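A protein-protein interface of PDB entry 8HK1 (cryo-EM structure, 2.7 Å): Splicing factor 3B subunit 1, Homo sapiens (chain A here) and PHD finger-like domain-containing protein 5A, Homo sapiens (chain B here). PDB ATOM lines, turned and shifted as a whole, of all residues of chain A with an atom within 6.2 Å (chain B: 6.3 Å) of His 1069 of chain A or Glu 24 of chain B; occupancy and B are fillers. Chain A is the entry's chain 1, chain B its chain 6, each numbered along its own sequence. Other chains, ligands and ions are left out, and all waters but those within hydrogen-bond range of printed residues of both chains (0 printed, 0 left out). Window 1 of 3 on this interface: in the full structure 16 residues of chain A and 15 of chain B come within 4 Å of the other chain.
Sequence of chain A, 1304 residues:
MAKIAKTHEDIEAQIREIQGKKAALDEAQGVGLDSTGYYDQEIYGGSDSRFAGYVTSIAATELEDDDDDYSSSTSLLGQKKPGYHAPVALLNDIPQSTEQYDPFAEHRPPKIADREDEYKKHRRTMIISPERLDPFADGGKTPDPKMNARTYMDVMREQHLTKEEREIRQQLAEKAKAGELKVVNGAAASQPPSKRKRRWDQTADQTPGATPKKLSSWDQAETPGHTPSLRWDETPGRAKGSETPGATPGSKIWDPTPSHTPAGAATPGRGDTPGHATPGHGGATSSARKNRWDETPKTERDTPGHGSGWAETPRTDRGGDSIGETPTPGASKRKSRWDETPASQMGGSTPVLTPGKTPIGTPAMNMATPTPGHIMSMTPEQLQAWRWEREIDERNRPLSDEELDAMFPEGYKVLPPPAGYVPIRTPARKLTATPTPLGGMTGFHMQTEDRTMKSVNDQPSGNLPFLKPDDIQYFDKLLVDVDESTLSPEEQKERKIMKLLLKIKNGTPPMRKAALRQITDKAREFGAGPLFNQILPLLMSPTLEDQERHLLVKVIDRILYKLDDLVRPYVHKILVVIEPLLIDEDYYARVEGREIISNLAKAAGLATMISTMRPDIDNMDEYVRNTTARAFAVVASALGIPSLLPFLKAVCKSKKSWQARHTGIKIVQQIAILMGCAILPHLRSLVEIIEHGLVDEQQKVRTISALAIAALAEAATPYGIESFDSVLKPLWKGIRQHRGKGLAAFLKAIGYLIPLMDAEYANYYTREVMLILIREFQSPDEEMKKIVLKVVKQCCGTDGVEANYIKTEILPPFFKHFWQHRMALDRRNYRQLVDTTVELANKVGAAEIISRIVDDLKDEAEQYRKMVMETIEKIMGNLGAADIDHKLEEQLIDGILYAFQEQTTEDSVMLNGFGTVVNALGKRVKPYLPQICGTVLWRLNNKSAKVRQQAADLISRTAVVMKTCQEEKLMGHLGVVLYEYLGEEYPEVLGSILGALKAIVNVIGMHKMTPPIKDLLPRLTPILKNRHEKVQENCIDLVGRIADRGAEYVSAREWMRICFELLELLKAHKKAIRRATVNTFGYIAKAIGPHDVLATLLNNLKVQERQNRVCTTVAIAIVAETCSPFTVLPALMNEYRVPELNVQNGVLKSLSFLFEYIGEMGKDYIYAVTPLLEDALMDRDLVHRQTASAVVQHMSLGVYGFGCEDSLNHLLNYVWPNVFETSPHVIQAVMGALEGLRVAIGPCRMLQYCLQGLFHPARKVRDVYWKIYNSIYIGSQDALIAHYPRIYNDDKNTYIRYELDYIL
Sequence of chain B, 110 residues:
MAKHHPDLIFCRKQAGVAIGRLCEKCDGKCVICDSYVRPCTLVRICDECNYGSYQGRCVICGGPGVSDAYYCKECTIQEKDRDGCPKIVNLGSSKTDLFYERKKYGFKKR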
ATOM      1  N   GLU A1029       0.977  14.119  39.045  1.00  0.00           N
ATOM      2  CA  GLU A1029       0.347  14.990  38.058  1.00  0.00           C
ATOM      3  C   GLU A1029      -0.664  15.930  38.704  1.00  0.00           C
ATOM      4  O   GLU A1029      -0.705  17.125  38.389  1.00  0.00           O
ATOM      5  CB  GLU A1029      -0.318  14.145  36.971  1.00  0.00           C
ATOM      6  CG  GLU A1029       0.543  12.994  36.485  1.00  0.00           C
ATOM      7  CD  GLU A1029       1.572  13.431  35.466  1.00  0.00           C
ATOM      8  OE1 GLU A1029       1.290  14.379  34.705  1.00  0.00           O
ATOM      9  OE2 GLU A1029       2.666  12.830  35.423  1.00  0.00           O
ATOM     10  N   LYS A1067       7.848  20.853  28.849  1.00  0.00           N
ATOM     11  CA  LYS A1067       8.127  19.583  28.193  1.00  0.00           C
ATOM     12  C   LYS A1067       7.271  18.442  28.724  1.00  0.00           C
ATOM     13  O   LYS A1067       7.464  17.299  28.302  1.00  0.00           O
ATOM     14  CB  LYS A1067       9.604  19.207  28.358  1.00  0.00           C
ATOM     15  CG  LYS A1067      10.511  20.361  28.723  1.00  0.00           C
ATOM     16  CD  LYS A1067      11.926  20.138  28.216  1.00  0.00           C
ATOM     17  CE  LYS A1067      12.673  19.140  29.082  1.00  0.00           C
ATOM     18  NZ  LYS A1067      14.079  18.969  28.638  1.00  0.00           N
ATOM     19  N   ALA A1068       6.355  18.724  29.650  1.00  0.00           N
ATOM     20  CA  ALA A1068       5.558  17.690  30.297  1.00  0.00           C
ATOM     21  C   ALA A1068       4.808  16.841  29.280  1.00  0.00           C
ATOM     22  O   ALA A1068       4.322  17.346  28.266  1.00  0.00           O
ATOM     23  CB  ALA A1068       4.572  18.331  31.274  1.00  0.00           C
ATOM     24  N   HIS A1069       4.720  15.541  29.564  1.00  0.00           N
ATOM     25  CA  HIS A1069       3.981  14.622  28.710  1.00  0.00           C
ATOM     26  C   HIS A1069       2.474  14.820  28.793  1.00  0.00           C
ATOM     27  O   HIS A1069       1.747  14.225  27.991  1.00  0.00           O
ATOM     28  CB  HIS A1069       4.330  13.177  29.075  1.00  0.00           C
ATOM     29  CG  HIS A1069       5.799  12.900  29.123  1.00  0.00           C
ATOM     30  ND1 HIS A1069       6.557  12.701  27.989  1.00  0.00           N
ATOM     31  CD2 HIS A1069       6.652  12.788  30.170  1.00  0.00           C
ATOM     32  CE1 HIS A1069       7.813  12.476  28.334  1.00  0.00           C
ATOM     33  NE2 HIS A1069       7.897  12.524  29.651  1.00  0.00           N
ATOM     34  N   LYS A1070       1.990  15.629  29.730  1.00  0.00           N
ATOM     35  CA  LYS A1070       0.564  15.792  29.981  1.00  0.00           C
ATOM     36  C   LYS A1070       0.120  17.182  29.546  1.00  0.00           C
ATOM     37  O   LYS A1070       0.872  18.151  29.688  1.00  0.00           O
ATOM     38  CB  LYS A1070       0.242  15.562  31.459  1.00  0.00           C
ATOM     39  CG  LYS A1070      -0.080  14.115  31.803  1.00  0.00           C
ATOM     40  CD  LYS A1070       1.135  13.213  31.620  1.00  0.00           C
ATOM     41  CE  LYS A1070       1.019  11.933  32.427  1.00  0.00           C
ATOM     42  NZ  LYS A1070       2.341  11.517  32.977  1.00  0.00           N
ATOM     43  N   LYS A1071      -1.105  17.273  29.027  1.00  0.00           N
ATOM     44  CA  LYS A1071      -1.569  18.518  28.419  1.00  0.00           C
ATOM     45  C   LYS A1071      -2.005  19.539  29.460  1.00  0.00           C
ATOM     46  O   LYS A1071      -1.832  20.747  29.255  1.00  0.00           O
ATOM     47  CB  LYS A1071      -2.711  18.216  27.449  1.00  0.00           C
ATOM     48  CG  LYS A1071      -2.989  19.313  26.444  1.00  0.00           C
ATOM     49  CD  LYS A1071      -4.472  19.604  26.345  1.00  0.00           C
ATOM     50  CE  LYS A1071      -5.160  18.622  25.416  1.00  0.00           C
ATOM     51  NZ  LYS A1071      -6.458  19.149  24.922  1.00  0.00           N
ATOM     52  N   ARG A1074       1.011  21.425  30.824  1.00  0.00           N
ATOM     53  CA  ARG A1074       1.485  22.432  29.883  1.00  0.00           C
ATOM     54  C   ARG A1074       0.557  23.641  29.840  1.00  0.00           C
ATOM     55  O   ARG A1074       1.019  24.784  29.782  1.00  0.00           O
ATOM     56  CB  ARG A1074       1.634  21.821  28.491  1.00  0.00           C
ATOM     57  CG  ARG A1074       2.679  20.727  28.405  1.00  0.00           C
ATOM     58  CD  ARG A1074       3.003  20.389  26.961  1.00  0.00           C
ATOM     59  NE  ARG A1074       1.811  20.015  26.206  1.00  0.00           N
ATOM     60  CZ  ARG A1074       1.491  18.766  25.887  1.00  0.00           C
ATOM     61  NH1 ARG A1074       2.278  17.764  26.254  1.00  0.00           N
ATOM     62  NH2 ARG A1074       0.385  18.516  25.200  1.00  0.00           N
ATOM     63  N   LEU B  22      -6.901  10.860  20.170  1.00  0.00           N
ATOM     64  CA  LEU B  22      -5.486  11.031  20.473  1.00  0.00           C
ATOM     65  C   LEU B  22      -5.175  10.388  21.814  1.00  0.00           C
ATOM     66  O   LEU B  22      -6.046  10.296  22.683  1.00  0.00           O
ATOM     67  CB  LEU B  22      -5.088  12.513  20.500  1.00  0.00           C
ATOM     68  CG  LEU B  22      -4.960  13.197  19.138  1.00  0.00           C
ATOM     69  CD1 LEU B  22      -4.677  14.679  19.290  1.00  0.00           C
ATOM     70  CD2 LEU B  22      -3.886  12.525  18.311  1.00  0.00           C
ATOM     71  N   CYS B  23      -3.931   9.947  21.979  1.00  0.00           N
ATOM     72  CA  CYS B  23      -3.522   9.308  23.220  1.00  0.00           C
ATOM     73  C   CYS B  23      -2.951  10.334  24.194  1.00  0.00           C
ATOM     74  O   CYS B  23      -2.915  11.538  23.924  1.00  0.00           O
ATOM     75  CB  CYS B  23      -2.495   8.208  22.948  1.00  0.00           C
ATOM     76  SG  CYS B  23      -0.834   8.798  22.581  1.00  0.00           S
ATOM     77  N   GLU B  24      -2.507   9.837  25.351  1.00  0.00           N
ATOM     78  CA  GLU B  24      -1.956  10.709  26.382  1.00  0.00           C
ATOM     79  C   GLU B  24      -0.660  11.377  25.949  1.00  0.00           C
ATOM     80  O   GLU B  24      -0.331  12.457  26.449  1.00  0.00           O
ATOM     81  CB  GLU B  24      -1.724   9.908  27.667  1.00  0.00           C
ATOM     82  CG  GLU B  24      -2.752  10.160  28.750  1.00  0.00           C
ATOM     83  CD  GLU B  24      -2.517  11.462  29.486  1.00  0.00           C
ATOM     84  OE1 GLU B  24      -1.350  11.747  29.834  1.00  0.00           O
ATOM     85  OE2 GLU B  24      -3.496  12.202  29.717  1.00  0.00           O
ATOM     86  N   LYS B  25       0.085  10.759  25.032  1.00  0.00           N
ATOM     87  CA  LYS B  25       1.355  11.332  24.600  1.00  0.00           C
ATOM     88  C   LYS B  25       1.162  12.335  23.468  1.00  0.00           C
ATOM     89  O   LYS B  25       1.927  13.300  23.349  1.00  0.00           O
ATOM     90  CB  LYS B  25       2.306  10.206  24.187  1.00  0.00           C
ATOM     91  CG  LYS B  25       3.654  10.665  23.669  1.00  0.00           C
ATOM     92  CD  LYS B  25       4.303   9.590  22.811  1.00  0.00           C
ATOM     93  CE  LYS B  25       3.388   9.156  21.678  1.00  0.00           C
ATOM     94  NZ  LYS B  25       4.035   8.152  20.790  1.00  0.00           N
ATOM     95  N   CYS B  26       0.142  12.137  22.633  1.00  0.00           N
ATOM     96  CA  CYS B  26      -0.102  12.969  21.461  1.00  0.00           C
ATOM     97  C   CYS B  26      -1.250  13.951  21.654  1.00  0.00           C
ATOM     98  O   CYS B  26      -1.749  14.498  20.667  1.00  0.00           O
ATOM     99  CB  CYS B  26      -0.389  12.088  20.244  1.00  0.00           C
ATOM    100  SG  CYS B  26       0.866  10.848  19.881  1.00  0.00           S
ATOM    101  N   ASP B  27      -1.670  14.195  22.898  1.00  0.00           N
ATOM    102  CA  ASP B  27      -2.975  14.802  23.163  1.00  0.00           C
ATOM    103  C   ASP B  27      -3.133  16.162  22.485  1.00  0.00           C
ATOM    104  O   ASP B  27      -4.202  16.476  21.951  1.00  0.00           O
ATOM    105  CB  ASP B  27      -3.185  14.921  24.673  1.00  0.00           C
ATOM    106  CG  ASP B  27      -4.636  15.153  25.043  1.00  0.00           C
ATOM    107  OD1 ASP B  27      -5.468  15.319  24.132  1.00  0.00           O
ATOM    108  OD2 ASP B  27      -4.945  15.166  26.251  1.00  0.00           O
ATOM    109  N   GLY B  28      -2.090  16.988  22.497  1.00  0.00           N
ATOM    110  CA  GLY B  28      -2.249  18.346  21.998  1.00  0.00           C
ATOM    111  C   GLY B  28      -1.838  18.516  20.546  1.00  0.00           C
ATOM    112  O   GLY B  28      -1.927  19.615  19.992  1.00  0.00           O
ATOM    113  N   PRO B  64      -4.018   3.646  22.987  1.00  0.00           N
ATOM    114  CA  PRO B  64      -5.394   3.878  23.446  1.00  0.00           C
ATOM    115  C   PRO B  64      -5.748   5.356  23.481  1.00  0.00           C
ATOM    116  O   PRO B  64      -5.067   6.152  24.132  1.00  0.00           O
ATOM    117  CB  PRO B  64      -5.404   3.262  24.851  1.00  0.00           C
ATOM    118  CG  PRO B  64      -3.985   3.297  25.287  1.00  0.00           C
ATOM    119  CD  PRO B  64      -3.159   3.103  24.054  1.00  0.00           C
ATOM    120  N   GLY B  65      -6.821   5.733  22.786  1.00  0.00           N
ATOM    121  CA  GLY B  65      -7.203   7.134  22.710  1.00  0.00           C
ATOM    122  C   GLY B  65      -7.810   7.627  24.015  1.00  0.00           C
ATOM    123  O   GLY B  65      -8.460   6.884  24.747  1.00  0.00           O
ATOM    124  N   VAL B  66      -7.580   8.907  24.303  1.00  0.00           N
ATOM    125  CA  VAL B  66      -8.132   9.545  25.494  1.00  0.00           C
ATOM    126  C   VAL B  66      -8.888  10.827  25.185  1.00  0.00           C
ATOM    127  O   VAL B  66      -9.723  11.242  26.004  1.00  0.00           O
ATOM    128  CB  VAL B  66      -7.039   9.824  26.549  1.00  0.00           C
ATOM    129  CG1 VAL B  66      -6.469   8.523  27.088  1.00  0.00           C
ATOM    130  CG2 VAL B  66      -5.943  10.693  25.966  1.00  0.00           C
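The backbone carbonyl oxygen of His 1069 of chain A lies close to the backbone carbonyl oxygen of Glu 24 of chain B (3.1 Å).
The side-chain carboxylate (OE2) of Glu 1029 of chain A lies within salt-bridge range of the side-chain amino group (NZ) of Lys 1070 of chain A, at 2.8 Å. O of Ala 1068 of chain A sits at hydrogen-bond distance from NH1 of Arg 1074 of chain A (2.9 Å).
Lys 1070 of chain A touches Glu 24 of chain B. CE of Lys 1071 of chain A touches CG of Asp 27 of chain B, at 3.5 Å. Arg 1074 of chain A touches Gly 28 of chain B (NH2 to N, 3.97 Å).
Of chain B, only Glu 24 (3.1 Å) comes within 4 Å of His 1069 of chain A. Glu 24 of chain B touches just these residues of chain A: His 1069 (3.1 Å) and Lys 1070 (3.3 Å). Of the printed residues of chain A, Gly 28 of chain B touches Arg 1074 (3.97 Å). Printed residues of chain B within 4 Å of Lys 1071 of chain A: Asp 27 (3.5 Å). Of the printed residues of chain B, Arg 1074 of chain A touches Gly 28 (3.97 Å). Cys 23 of chain B touches none of the printed residues of chain A. Gly 65 of chain B touches none of the printed residues of chain A. The nearest residue of chain B that does not touch His 1069 of chain A is Lys 25 of chain B (4.5 Å). The nearest printed residue of chain B that does not touch Lys 1070 of chain A is Asp 27 of chain B (6.3 Å).
Along chain A the printed residues that touch a printed residue of chain B span positions 1069 to 1074. Printed residues of chain B that touch a printed residue of chain A: Glu 24, Asp 27 and Gly 28. Among the printed residues, no Asp or Glu carboxylate lies within 4 Å of a Lys or Arg side-chain nitrogen of the other chain.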
